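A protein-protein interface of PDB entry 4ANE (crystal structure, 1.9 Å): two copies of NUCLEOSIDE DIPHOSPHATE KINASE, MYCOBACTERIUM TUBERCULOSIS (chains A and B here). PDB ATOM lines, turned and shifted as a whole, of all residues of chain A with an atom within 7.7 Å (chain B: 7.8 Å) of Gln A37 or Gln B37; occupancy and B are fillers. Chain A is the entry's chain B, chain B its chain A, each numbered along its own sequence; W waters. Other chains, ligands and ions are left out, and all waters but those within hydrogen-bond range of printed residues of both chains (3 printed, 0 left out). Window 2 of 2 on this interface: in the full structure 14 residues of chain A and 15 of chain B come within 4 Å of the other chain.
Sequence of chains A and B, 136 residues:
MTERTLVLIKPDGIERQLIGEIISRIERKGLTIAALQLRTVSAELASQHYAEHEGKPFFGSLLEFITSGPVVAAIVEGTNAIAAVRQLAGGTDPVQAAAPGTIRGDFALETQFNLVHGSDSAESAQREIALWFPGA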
ATOM      1  N   VAL A   7      -2.239 -14.969  -3.370  1.00  0.00           N
ATOM      2  CA  VAL A   7      -2.769 -13.622  -3.502  1.00  0.00           C
ATOM      3  C   VAL A   7      -2.241 -12.769  -2.368  1.00  0.00           C
ATOM      4  O   VAL A   7      -2.196 -13.207  -1.211  1.00  0.00           O
ATOM      5  CB  VAL A   7      -4.318 -13.626  -3.451  1.00  0.00           C
ATOM      6  CG1 VAL A   7      -4.866 -12.206  -3.361  1.00  0.00           C
ATOM      7  CG2 VAL A   7      -4.883 -14.348  -4.666  1.00  0.00           C
ATOM      8  N   LEU A   8      -1.809 -11.561  -2.699  1.00  0.00           N
ATOM      9  CA  LEU A   8      -1.397 -10.595  -1.689  1.00  0.00           C
ATOM     10  C   LEU A   8      -2.233  -9.361  -1.859  1.00  0.00           C
ATOM     11  O   LEU A   8      -2.384  -8.853  -2.968  1.00  0.00           O
ATOM     12  CB  LEU A   8       0.064 -10.172  -1.867  1.00  0.00           C
ATOM     13  CG  LEU A   8       1.203 -11.125  -1.587  1.00  0.00           C
ATOM     14  CD1 LEU A   8       2.512 -10.361  -1.772  1.00  0.00           C
ATOM     15  CD2 LEU A   8       1.085 -11.687  -0.181  1.00  0.00           C
ATOM     16  N   ILE A   9      -2.789  -8.888  -0.759  1.00  0.00           N
ATOM     17  CA  ILE A   9      -3.400  -7.582  -0.742  1.00  0.00           C
ATOM     18  C   ILE A   9      -2.333  -6.699  -0.146  1.00  0.00           C
ATOM     19  O   ILE A   9      -1.936  -6.882   1.003  1.00  0.00           O
ATOM     20  CB  ILE A   9      -4.679  -7.547   0.094  1.00  0.00           C
ATOM     21  CG1 ILE A   9      -5.692  -8.530  -0.488  1.00  0.00           C
ATOM     22  CG2 ILE A   9      -5.256  -6.113   0.124  1.00  0.00           C
ATOM     23  CD1 ILE A   9      -7.001  -8.621   0.272  1.00  0.00           C
ATOM     24  N   ILE A  14      -5.065  -2.445   2.020  1.00  0.00           N
ATOM     25  CA  ILE A  14      -5.486  -2.441   3.426  1.00  0.00           C
ATOM     26  C   ILE A  14      -5.861  -1.028   3.882  1.00  0.00           C
ATOM     27  O   ILE A  14      -6.932  -0.803   4.449  1.00  0.00           O
ATOM     28  CB  ILE A  14      -4.402  -3.031   4.335  1.00  0.00           C
ATOM     29  CG1 ILE A  14      -4.190  -4.512   3.991  1.00  0.00           C
ATOM     30  CG2 ILE A  14      -4.777  -2.856   5.802  1.00  0.00           C
ATOM     31  CD1 ILE A  14      -3.222  -5.189   4.890  1.00  0.00           C
ATOM     32  N   ILE A  33     -10.908 -19.721  -0.420  1.00  0.00           N
ATOM     33  CA  ILE A  33      -9.790 -19.222   0.347  1.00  0.00           C
ATOM     34  C   ILE A  33      -9.301 -20.365   1.201  1.00  0.00           C
ATOM     35  O   ILE A  33      -9.973 -20.761   2.152  1.00  0.00           O
ATOM     36  CB  ILE A  33     -10.241 -18.087   1.260  1.00  0.00           C
ATOM     37  CG1 ILE A  33     -10.970 -17.012   0.441  1.00  0.00           C
ATOM     38  CG2 ILE A  33      -9.057 -17.538   2.047  1.00  0.00           C
ATOM     39  CD1 ILE A  33     -10.106 -16.387  -0.657  1.00  0.00           C
ATOM     40  N   ALA A  35      -6.170 -20.428   2.717  1.00  0.00           N
ATOM     41  CA  ALA A  35      -5.347 -19.916   3.812  1.00  0.00           C
ATOM     42  C   ALA A  35      -5.409 -18.402   3.761  1.00  0.00           C
ATOM     43  O   ALA A  35      -5.564 -17.833   2.696  1.00  0.00           O
ATOM     44  CB  ALA A  35      -3.911 -20.395   3.679  1.00  0.00           C
ATOM     45  N   LEU A  36      -5.292 -17.748   4.911  1.00  0.00           N
ATOM     46  CA  LEU A  36      -5.517 -16.314   4.952  1.00  0.00           C
ATOM     47  C   LEU A  36      -4.853 -15.750   6.194  1.00  0.00           C
ATOM     48  O   LEU A  36      -5.049 -16.271   7.286  1.00  0.00           O
ATOM     49  CB  LEU A  36      -7.030 -16.029   4.977  1.00  0.00           C
ATOM     50  CG  LEU A  36      -7.429 -14.552   5.082  1.00  0.00           C
ATOM     51  CD1 LEU A  36      -7.080 -13.899   3.770  1.00  0.00           C
ATOM     52  CD2 LEU A  36      -8.914 -14.393   5.373  1.00  0.00           C
ATOM     53  N   GLN A  37      -4.033 -14.718   6.027  1.00  0.00           N
ATOM     54  CA  GLN A  37      -3.356 -14.108   7.177  1.00  0.00           C
ATOM     55  C   GLN A  37      -2.904 -12.676   6.932  1.00  0.00           C
ATOM     56  O   GLN A  37      -2.303 -12.357   5.899  1.00  0.00           O
ATOM     57  CB  GLN A  37      -2.169 -14.959   7.671  1.00  0.00           C
ATOM     58  CG  GLN A  37      -1.620 -14.518   9.062  1.00  0.00           C
ATOM     59  CD  GLN A  37      -0.680 -15.543   9.696  1.00  0.00           C
ATOM     60  OE1 GLN A  37      -0.858 -16.748   9.540  1.00  0.00           O
ATOM     61  NE2 GLN A  37       0.327 -15.061  10.413  1.00  0.00           N
ATOM     62  N   LEU A  38      -3.226 -11.814   7.892  1.00  0.00           N
ATOM     63  CA  LEU A  38      -2.702 -10.458   7.931  1.00  0.00           C
ATOM     64  C   LEU A  38      -1.309 -10.523   8.520  1.00  0.00           C
ATOM     65  O   LEU A  38      -1.108 -11.095   9.592  1.00  0.00           O
ATOM     66  CB  LEU A  38      -3.578  -9.587   8.827  1.00  0.00           C
ATOM     67  CG  LEU A  38      -3.130  -8.150   9.071  1.00  0.00           C
ATOM     68  CD1 LEU A  38      -3.217  -7.355   7.783  1.00  0.00           C
ATOM     69  CD2 LEU A  38      -3.984  -7.511  10.155  1.00  0.00           C
ATOM     70  N   ARG A  39      -0.334  -9.933   7.841  1.00  0.00           N
ATOM     71  CA  ARG A  39       1.022  -9.979   8.377  1.00  0.00           C
ATOM     72  C   ARG A  39       1.911  -8.811   7.972  1.00  0.00           C
ATOM     73  O   ARG A  39       1.626  -8.101   7.013  1.00  0.00           O
ATOM     74  CB  ARG A  39       1.687 -11.308   8.037  1.00  0.00           C
ATOM     75  CG  ARG A  39       1.644 -11.662   6.579  1.00  0.00           C
ATOM     76  CD  ARG A  39       2.253 -13.024   6.358  1.00  0.00           C
ATOM     77  NE  ARG A  39       3.638 -13.064   6.811  1.00  0.00           N
ATOM     78  CZ  ARG A  39       4.446 -14.106   6.657  1.00  0.00           C
ATOM     79  NH1 ARG A  39       4.014 -15.209   6.060  1.00  0.00           N
ATOM     80  NH2 ARG A  39       5.692 -14.042   7.101  1.00  0.00           N
ATOM     81  N   THR A  40       2.980  -8.613   8.735  1.00  0.00           N
ATOM     82  CA  THR A  40       4.007  -7.644   8.375  1.00  0.00           C
ATOM     83  C   THR A  40       5.069  -8.350   7.538  1.00  0.00           C
ATOM     84  O   THR A  40       5.310  -9.542   7.704  1.00  0.00           O
ATOM     85  CB  THR A  40       4.660  -7.030   9.613  1.00  0.00           C
ATOM     86  OG1 THR A  40       5.617  -6.047   9.205  1.00  0.00           O
ATOM     87  CG2 THR A  40       5.351  -8.106  10.430  1.00  0.00           C
ATOM     88  N   PRO A  70       1.223  -3.481   6.892  1.00  0.00           N
ATOM     89  CA  PRO A  70       0.770  -4.871   6.831  1.00  0.00           C
ATOM     90  C   PRO A  70       0.206  -5.233   5.454  1.00  0.00           C
ATOM     91  O   PRO A  70      -0.273  -4.371   4.717  1.00  0.00           O
ATOM     92  CB  PRO A  70      -0.338  -4.918   7.884  1.00  0.00           C
ATOM     93  CG  PRO A  70      -0.814  -3.506   7.990  1.00  0.00           C
ATOM     94  CD  PRO A  70       0.412  -2.674   7.818  1.00  0.00           C
ATOM     95  N   VAL A  71       0.292  -6.507   5.106  1.00  0.00           N
ATOM     96  CA  VAL A  71      -0.391  -7.024   3.922  1.00  0.00           C
ATOM     97  C   VAL A  71      -1.255  -8.185   4.339  1.00  0.00           C
ATOM     98  O   VAL A  71      -1.085  -8.728   5.430  1.00  0.00           O
ATOM     99  CB  VAL A  71       0.586  -7.555   2.848  1.00  0.00           C
ATOM    100  CG1 VAL A  71       1.574  -6.480   2.417  1.00  0.00           C
ATOM    101  CG2 VAL A  71       1.312  -8.797   3.351  1.00  0.00           C
ATOM    102  N   VAL A  72      -2.174  -8.578   3.468  1.00  0.00           N
ATOM    103  CA  VAL A  72      -2.902  -9.816   3.668  1.00  0.00           C
ATOM    104  C   VAL A  72      -2.472 -10.824   2.607  1.00  0.00           C
ATOM    105  O   VAL A  72      -2.515 -10.539   1.408  1.00  0.00           O
ATOM    106  CB  VAL A  72      -4.430  -9.607   3.596  1.00  0.00           C
ATOM    107  CG1 VAL A  72      -5.141 -10.949   3.432  1.00  0.00           C
ATOM    108  CG2 VAL A  72      -4.935  -8.862   4.845  1.00  0.00           C
ATOM    109  N   ALA A  73      -2.046 -11.998   3.055  1.00  0.00           N
ATOM    110  CA  ALA A  73      -1.656 -13.074   2.146  1.00  0.00           C
ATOM    111  C   ALA A  73      -2.727 -14.146   2.161  1.00  0.00           C
ATOM    112  O   ALA A  73      -3.308 -14.437   3.214  1.00  0.00           O
ATOM    113  CB  ALA A  73      -0.314 -13.662   2.577  1.00  0.00           C
ATOM    114  N   ALA A  74      -3.001 -14.739   1.002  1.00  0.00           N
ATOM    115  CA  ALA A  74      -3.989 -15.799   0.942  1.00  0.00           C
ATOM    116  C   ALA A  74      -3.587 -16.875  -0.051  1.00  0.00           C
ATOM    117  O   ALA A  74      -2.996 -16.586  -1.093  1.00  0.00           O
ATOM    118  CB  ALA A  74      -5.360 -15.230   0.574  1.00  0.00           C
ATOM    119  N   ILE A  75      -3.911 -18.120   0.273  1.00  0.00           N
ATOM    120  CA  ILE A  75      -3.902 -19.165  -0.743  1.00  0.00           C
ATOM    121  C   ILE A  75      -5.305 -19.273  -1.311  1.00  0.00           C
ATOM    122  O   ILE A  75      -6.276 -19.458  -0.567  1.00  0.00           O
ATOM    123  CB  ILE A  75      -3.467 -20.539  -0.179  1.00  0.00           C
ATOM    124  CG1 ILE A  75      -2.038 -20.481   0.369  1.00  0.00           C
ATOM    125  CG2 ILE A  75      -3.586 -21.614  -1.264  1.00  0.00           C
ATOM    126  CD1 ILE A  75      -1.629 -21.772   1.041  1.00  0.00           C
ATOM    127  N   TRP A 132       5.423 -17.822   1.333  1.00  0.00           N
ATOM    128  CA  TRP A 132       4.486 -17.171   2.252  1.00  0.00           C
ATOM    129  C   TRP A 132       3.774 -18.122   3.215  1.00  0.00           C
ATOM    130  O   TRP A 132       3.410 -17.740   4.332  1.00  0.00           O
ATOM    131  CB  TRP A 132       3.440 -16.381   1.471  1.00  0.00           C
ATOM    132  CG  TRP A 132       3.986 -15.163   0.843  1.00  0.00           C
ATOM    133  CD1 TRP A 132       4.594 -15.067  -0.374  1.00  0.00           C
ATOM    134  CD2 TRP A 132       3.982 -13.850   1.401  1.00  0.00           C
ATOM    135  NE1 TRP A 132       4.967 -13.767  -0.610  1.00  0.00           N
ATOM    136  CE2 TRP A 132       4.599 -13.003   0.461  1.00  0.00           C
ATOM    137  CE3 TRP A 132       3.513 -13.312   2.599  1.00  0.00           C
ATOM    138  CZ2 TRP A 132       4.759 -11.640   0.691  1.00  0.00           C
ATOM    139  CZ3 TRP A 132       3.672 -11.961   2.823  1.00  0.00           C
ATOM    140  CH2 TRP A 132       4.285 -11.139   1.871  1.00  0.00           C
ATOM    141  N   PHE A 133       3.556 -19.356   2.780  1.00  0.00           N
ATOM    142  CA  PHE A 133       2.870 -20.338   3.612  1.00  0.00           C
ATOM    143  C   PHE A 133       3.616 -21.674   3.586  1.00  0.00           C
ATOM    144  O   PHE A 133       3.036 -22.693   3.211  1.00  0.00           O
ATOM    145  CB  PHE A 133       1.426 -20.583   3.129  1.00  0.00           C
ATOM    146  CG  PHE A 133       0.496 -19.391   3.258  1.00  0.00           C
ATOM    147  CD1 PHE A 133      -0.216 -19.167   4.433  1.00  0.00           C
ATOM    148  CD2 PHE A 133       0.302 -18.532   2.191  1.00  0.00           C
ATOM    149  CE1 PHE A 133      -1.088 -18.083   4.544  1.00  0.00           C
ATOM    150  CE2 PHE A 133      -0.580 -17.447   2.281  1.00  0.00           C
ATOM    151  CZ  PHE A 133      -1.268 -17.217   3.468  1.00  0.00           C
ATOM    152  N   VAL B   7     -13.594 -11.130  16.463  1.00  0.00           N
ATOM    153  CA  VAL B   7     -14.606 -11.551  15.508  1.00  0.00           C
ATOM    154  C   VAL B   7     -14.237 -12.926  14.965  1.00  0.00           C
ATOM    155  O   VAL B   7     -13.074 -13.188  14.673  1.00  0.00           O
ATOM    156  CB  VAL B   7     -14.728 -10.545  14.317  1.00  0.00           C
ATOM    157  CG1 VAL B   7     -15.589 -11.121  13.211  1.00  0.00           C
ATOM    158  CG2 VAL B   7     -15.282  -9.214  14.789  1.00  0.00           C
ATOM    159  N   LEU B   8     -15.226 -13.810  14.865  1.00  0.00           N
ATOM    160  CA  LEU B   8     -15.014 -15.135  14.300  1.00  0.00           C
ATOM    161  C   LEU B   8     -15.964 -15.286  13.130  1.00  0.00           C
ATOM    162  O   LEU B   8     -17.150 -15.009  13.250  1.00  0.00           O
ATOM    163  CB  LEU B   8     -15.326 -16.249  15.315  1.00  0.00           C
ATOM    164  CG  LEU B   8     -14.427 -16.552  16.505  1.00  0.00           C
ATOM    165  CD1 LEU B   8     -14.990 -17.757  17.291  1.00  0.00           C
ATOM    166  CD2 LEU B   8     -13.012 -16.823  16.034  1.00  0.00           C
ATOM    167  N   ILE B   9     -15.441 -15.706  11.989  1.00  0.00           N
ATOM    168  CA  ILE B   9     -16.319 -16.176  10.930  1.00  0.00           C
ATOM    169  C   ILE B   9     -16.366 -17.683  11.082  1.00  0.00           C
ATOM    170  O   ILE B   9     -15.329 -18.337  11.027  1.00  0.00           O
ATOM    171  CB  ILE B   9     -15.821 -15.752   9.554  1.00  0.00           C
ATOM    172  CG1 ILE B   9     -15.692 -14.220   9.519  1.00  0.00           C
ATOM    173  CG2 ILE B   9     -16.794 -16.228   8.476  1.00  0.00           C
ATOM    174  CD1 ILE B   9     -15.058 -13.657   8.231  1.00  0.00           C
ATOM    175  N   ILE B  14     -17.603 -19.531   6.092  1.00  0.00           N
ATOM    176  CA  ILE B  14     -16.601 -19.876   5.090  1.00  0.00           C
ATOM    177  C   ILE B  14     -17.201 -20.735   3.978  1.00  0.00           C
ATOM    178  O   ILE B  14     -16.974 -20.473   2.792  1.00  0.00           O
ATOM    179  CB  ILE B  14     -15.384 -20.578   5.718  1.00  0.00           C
ATOM    180  CG1 ILE B  14     -14.683 -19.628   6.687  1.00  0.00           C
ATOM    181  CG2 ILE B  14     -14.393 -21.038   4.641  1.00  0.00           C
ATOM    182  CD1 ILE B  14     -13.309 -20.074   7.059  1.00  0.00           C
ATOM    183  N   ILE B  33      -9.135  -3.933  10.571  1.00  0.00           N
ATOM    184  CA  ILE B  33      -8.750  -5.321  10.821  1.00  0.00           C
ATOM    185  C   ILE B  33      -7.317  -5.327  11.361  1.00  0.00           C
ATOM    186  O   ILE B  33      -6.378  -5.073  10.615  1.00  0.00           O
ATOM    187  CB  ILE B  33      -8.790  -6.159   9.507  1.00  0.00           C
ATOM    188  CG1 ILE B  33     -10.139  -6.017   8.803  1.00  0.00           C
ATOM    189  CG2 ILE B  33      -8.438  -7.653   9.776  1.00  0.00           C
ATOM    190  CD1 ILE B  33     -11.327  -6.473   9.641  1.00  0.00           C
ATOM    191  N   ALA B  35      -5.880  -7.934  13.085  1.00  0.00           N
ATOM    192  CA  ALA B  35      -5.301  -9.266  12.939  1.00  0.00           C
ATOM    193  C   ALA B  35      -6.342 -10.116  12.237  1.00  0.00           C
ATOM    194  O   ALA B  35      -7.539  -9.821  12.307  1.00  0.00           O
ATOM    195  CB  ALA B  35      -4.916  -9.868  14.301  1.00  0.00           C
ATOM    196  N   LEU B  36      -5.877 -11.145  11.536  1.00  0.00           N
ATOM    197  CA  LEU B  36      -6.739 -11.940  10.672  1.00  0.00           C
ATOM    198  C   LEU B  36      -6.053 -13.262  10.362  1.00  0.00           C
ATOM    199  O   LEU B  36      -4.908 -13.286   9.889  1.00  0.00           O
ATOM    200  CB  LEU B  36      -7.010 -11.189   9.367  1.00  0.00           C
ATOM    201  CG  LEU B  36      -7.982 -11.787   8.344  1.00  0.00           C
ATOM    202  CD1 LEU B  36      -9.404 -11.773   8.886  1.00  0.00           C
ATOM    203  CD2 LEU B  36      -7.904 -11.011   7.029  1.00  0.00           C
ATOM    204  N   GLN B  37      -6.751 -14.362  10.617  1.00  0.00           N
ATOM    205  CA  GLN B  37      -6.193 -15.678  10.322  1.00  0.00           C
ATOM    206  C   GLN B  37      -7.247 -16.752  10.088  1.00  0.00           C
ATOM    207  O   GLN B  37      -8.162 -16.921  10.882  1.00  0.00           O
ATOM    208  CB  GLN B  37      -5.250 -16.152  11.436  1.00  0.00           C
ATOM    209  CG  GLN B  37      -4.603 -17.511  11.105  1.00  0.00           C
ATOM    210  CD  GLN B  37      -3.831 -18.141  12.256  1.00  0.00           C
ATOM    211  OE1 GLN B  37      -4.313 -18.221  13.382  1.00  0.00           O
ATOM    212  NE2 GLN B  37      -2.626 -18.613  11.961  1.00  0.00           N
ATOM    213  N   LEU B  38      -7.105 -17.475   8.985  1.00  0.00           N
ATOM    214  CA  LEU B  38      -7.906 -18.665   8.743  1.00  0.00           C
ATOM    215  C   LEU B  38      -7.227 -19.818   9.475  1.00  0.00           C
ATOM    216  O   LEU B  38      -6.025 -20.039   9.314  1.00  0.00           O
ATOM    217  CB  LEU B  38      -7.995 -18.956   7.238  1.00  0.00           C
ATOM    218  CG  LEU B  38      -8.979 -20.050   6.813  1.00  0.00           C
ATOM    219  CD1 LEU B  38      -9.407 -19.871   5.357  1.00  0.00           C
ATOM    220  CD2 LEU B  38      -8.399 -21.438   7.051  1.00  0.00           C
ATOM    221  N   ARG B  39      -7.984 -20.552  10.286  1.00  0.00           N
ATOM    222  CA  ARG B  39      -7.395 -21.611  11.104  1.00  0.00           C
ATOM    223  C   ARG B  39      -8.383 -22.717  11.451  1.00  0.00           C
ATOM    224  O   ARG B  39      -9.597 -22.540  11.335  1.00  0.00           O
ATOM    225  CB  ARG B  39      -6.871 -21.003  12.403  1.00  0.00           C
ATOM    226  CG  ARG B  39      -7.949 -20.240  13.171  1.00  0.00           C
ATOM    227  CD  ARG B  39      -7.404 -19.628  14.458  1.00  0.00           C
ATOM    228  NE  ARG B  39      -6.845 -20.633  15.356  1.00  0.00           N
ATOM    229  CZ  ARG B  39      -6.403 -20.385  16.587  1.00  0.00           C
ATOM    230  NH1 ARG B  39      -6.449 -19.159  17.084  1.00  0.00           N
ATOM    231  NH2 ARG B  39      -5.905 -21.368  17.320  1.00  0.00           N
ATOM    232  N   THR B  40      -7.856 -23.851  11.905  1.00  0.00           N
ATOM    233  CA  THR B  40      -8.698 -24.908  12.422  1.00  0.00           C
ATOM    234  C   THR B  40      -8.789 -24.720  13.932  1.00  0.00           C
ATOM    235  O   THR B  40      -7.883 -24.174  14.557  1.00  0.00           O
ATOM    236  CB  THR B  40      -8.116 -26.300  12.125  1.00  0.00           C
ATOM    237  OG1 THR B  40      -6.742 -26.316  12.516  1.00  0.00           O
ATOM    238  CG2 THR B  40      -8.217 -26.620  10.641  1.00  0.00           C
ATOM    239  N   PRO B  70     -12.757 -25.065   8.966  1.00  0.00           N
ATOM    240  CA  PRO B  70     -11.949 -23.890   9.294  1.00  0.00           C
ATOM    241  C   PRO B  70     -12.815 -22.694   9.668  1.00  0.00           C
ATOM    242  O   PRO B  70     -13.982 -22.581   9.264  1.00  0.00           O
ATOM    243  CB  PRO B  70     -11.180 -23.615   7.993  1.00  0.00           C
ATOM    244  CG  PRO B  70     -11.987 -24.258   6.926  1.00  0.00           C
ATOM    245  CD  PRO B  70     -12.588 -25.485   7.565  1.00  0.00           C
ATOM    246  N   VAL B  71     -12.241 -21.809  10.463  1.00  0.00           N
ATOM    247  CA  VAL B  71     -12.885 -20.537  10.763  1.00  0.00           C
ATOM    248  C   VAL B  71     -11.916 -19.411  10.434  1.00  0.00           C
ATOM    249  O   VAL B  71     -10.715 -19.629  10.301  1.00  0.00           O
ATOM    250  CB  VAL B  71     -13.286 -20.427  12.253  1.00  0.00           C
ATOM    251  CG1 VAL B  71     -14.102 -21.643  12.687  1.00  0.00           C
ATOM    252  CG2 VAL B  71     -12.048 -20.292  13.132  1.00  0.00           C
ATOM    253  N   VAL B  72     -12.444 -18.201  10.317  1.00  0.00           N
ATOM    254  CA  VAL B  72     -11.587 -17.038  10.268  1.00  0.00           C
ATOM    255  C   VAL B  72     -11.683 -16.252  11.579  1.00  0.00           C
ATOM    256  O   VAL B  72     -12.765 -15.825  11.972  1.00  0.00           O
ATOM    257  CB  VAL B  72     -11.951 -16.117   9.102  1.00  0.00           C
ATOM    258  CG1 VAL B  72     -11.085 -14.893   9.147  1.00  0.00           C
ATOM    259  CG2 VAL B  72     -11.783 -16.850   7.759  1.00  0.00           C
ATOM    260  N   ALA B  73     -10.549 -16.067  12.247  1.00  0.00           N
ATOM    261  CA  ALA B  73     -10.489 -15.216  13.444  1.00  0.00           C
ATOM    262  C   ALA B  73      -9.854 -13.862  13.124  1.00  0.00           C
ATOM    263  O   ALA B  73      -8.887 -13.782  12.363  1.00  0.00           O
ATOM    264  CB  ALA B  73      -9.713 -15.907  14.546  1.00  0.00           C
ATOM    265  N   ALA B  74     -10.406 -12.805  13.708  1.00  0.00           N
ATOM    266  CA  ALA B  74      -9.936 -11.450  13.463  1.00  0.00           C
ATOM    267  C   ALA B  74      -9.965 -10.616  14.732  1.00  0.00           C
ATOM    268  O   ALA B  74     -10.863 -10.763  15.564  1.00  0.00           O
ATOM    269  CB  ALA B  74     -10.785 -10.770  12.407  1.00  0.00           C
ATOM    270  N   ILE B  75      -8.988  -9.729  14.869  1.00  0.00           N
ATOM    271  CA  ILE B  75      -9.114  -8.665  15.849  1.00  0.00           C
ATOM    272  C   ILE B  75      -9.589  -7.429  15.108  1.00  0.00           C
ATOM    273  O   ILE B  75      -8.974  -7.003  14.122  1.00  0.00           O
ATOM    274  CB  ILE B  75      -7.810  -8.353  16.606  1.00  0.00           C
ATOM    275  CG1 ILE B  75      -7.368  -9.553  17.448  1.00  0.00           C
ATOM    276  CG2 ILE B  75      -8.037  -7.146  17.533  1.00  0.00           C
ATOM    277  CD1 ILE B  75      -5.980  -9.401  18.095  1.00  0.00           C
ATOM    278  N   TRP B 132      -7.573 -16.369  21.495  1.00  0.00           N
ATOM    279  CA  TRP B 132      -7.369 -16.601  20.057  1.00  0.00           C
ATOM    280  C   TRP B 132      -6.058 -16.011  19.521  1.00  0.00           C
ATOM    281  O   TRP B 132      -5.467 -16.543  18.574  1.00  0.00           O
ATOM    282  CB  TRP B 132      -8.570 -16.066  19.259  1.00  0.00           C
ATOM    283  CG  TRP B 132      -9.848 -16.894  19.438  1.00  0.00           C
ATOM    284  CD1 TRP B 132     -10.746 -16.827  20.478  1.00  0.00           C
ATOM    285  CD2 TRP B 132     -10.327 -17.917  18.564  1.00  0.00           C
ATOM    286  NE1 TRP B 132     -11.768 -17.738  20.284  1.00  0.00           N
ATOM    287  CE2 TRP B 132     -11.532 -18.418  19.116  1.00  0.00           C
ATOM    288  CE3 TRP B 132      -9.860 -18.458  17.352  1.00  0.00           C
ATOM    289  CZ2 TRP B 132     -12.270 -19.437  18.504  1.00  0.00           C
ATOM    290  CZ3 TRP B 132     -10.599 -19.455  16.745  1.00  0.00           C
ATOM    291  CH2 TRP B 132     -11.790 -19.942  17.326  1.00  0.00           C
ATOM    292  N   PHE B 133      -5.614 -14.915  20.130  1.00  0.00           N
ATOM    293  CA  PHE B 133      -4.427 -14.196  19.678  1.00  0.00           C
ATOM    294  C   PHE B 133      -3.543 -13.850  20.866  1.00  0.00           C
ATOM    295  O   PHE B 133      -3.383 -12.681  21.210  1.00  0.00           O
ATOM    296  CB  PHE B 133      -4.827 -12.917  18.928  1.00  0.00           C
ATOM    297  CG  PHE B 133      -5.521 -13.172  17.625  1.00  0.00           C
ATOM    298  CD1 PHE B 133      -4.798 -13.610  16.519  1.00  0.00           C
ATOM    299  CD2 PHE B 133      -6.884 -12.965  17.489  1.00  0.00           C
ATOM    300  CE1 PHE B 133      -5.420 -13.847  15.299  1.00  0.00           C
ATOM    301  CE2 PHE B 133      -7.520 -13.194  16.260  1.00  0.00           C
ATOM    302  CZ  PHE B 133      -6.783 -13.635  15.167  1.00  0.00           C
HETATM  303  O   HOH W   1      -4.567 -19.449   7.066  1.00  0.00           O
HETATM  304  O   HOH W   2      -2.193 -19.040   8.550  1.00  0.00           O
HETATM  305  O   HOH W   3      -2.821 -11.330  11.727  1.00  0.00           O
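The backbone NH (N) of Leu A38 is in hydrogen-bond range of the backbone carbonyl oxygen (O) of Leu B36 (3.0 Å).
The backbone NH of Leu B38 lies within hydrogen-bond range of the backbone carbonyl oxygen of Leu A36 (2.9 Å).
O of Ala B35 sits at hydrogen-bond distance from N of Ile B75, 2.9 Å away.
The backbone NH of Gln B37 is in hydrogen-bond range of the backbone carbonyl oxygen of Ala B73 (2.8 Å).
O of Gln A37 is in hydrogen-bond range of N of Ala A73, 2.9 Å away.
Among the printed residues, pairs that only touch across the chains: Ile A33 with Leu B38 (3.4 Å), Leu A36 with Leu B36 (3.9 Å), Leu A36 with Gln B37 (3.3 Å), Gln A37 with Leu B36 (3.2 Å), Gln A37 with Gln B37 (3.5 Å), Leu A38 with Ile B33 (3.4 Å) and Leu A38 with Ala B35 (3.5 Å).
Gln A37 touches just these residues of chain B: Leu B36 (3.2 Å) and Gln B37 (3.5 Å).
Of the printed residues of chain A, Ala B35 touches Leu A38 (3.5 Å).
Printed residues of chain A within 4 Å of Ile B33: Leu A38.
Of the printed residues of chain A, Leu B36 touches Leu A36, Gln A37 and Leu A38.
Of the printed residues of chain A, Leu B38 touches Ile A33 (3.4 Å) and Leu A36 (2.9 Å).
Phe B133 touches none of the printed residues of chain A.
The nearest printed residue of chain B that does not touch Gln A37 is Leu B38 (5.1 Å).
The nearest residue of chain A that does not touch Gln B37 is Leu A38 (5.1 Å).
The nearest printed residue of chain A that does not touch Ile B33 is Ile A14 (5.5 Å).
Of the 19 printed residues of chain B, 5 touch a printed residue of chain A.
Of the 19 printed residues of chain A, 4 touch a printed residue of chain B.
Printed residues of chain A that touch a printed residue of chain B: Ile A33, Leu A36, Gln A37 and Leu A38.
Hydrophobic or aromatic side chains of chain A that line the printed part of chain B: Leu A36 and Leu A38.
Leu B36 touches its own counterpart, Leu A36.
Leu A36 touches Gln B37, and with the chains exchanged Gln A37 touches Leu B36.
Leu A36 touches Leu B38, and with the chains exchanged Leu A38 touches Leu B36.
Gln A37 touches its own counterpart, Gln B37.
Of the 9 pairs that touch across the chains among the printed residues, 8 have their exchanged pair printed and touching as well.
Water W1 bridges O of Leu B38 (2.7 Å) and N of Leu A36 (2.8 Å).
Water W3 lies within hydrogen-bond range of O of Leu A38 (2.7 Å) and N of Leu B36 (3.1 Å).
Water W2 bridges OE1 of Gln A37 (2.8 Å) and NE2 of Gln B37 (3.5 Å).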
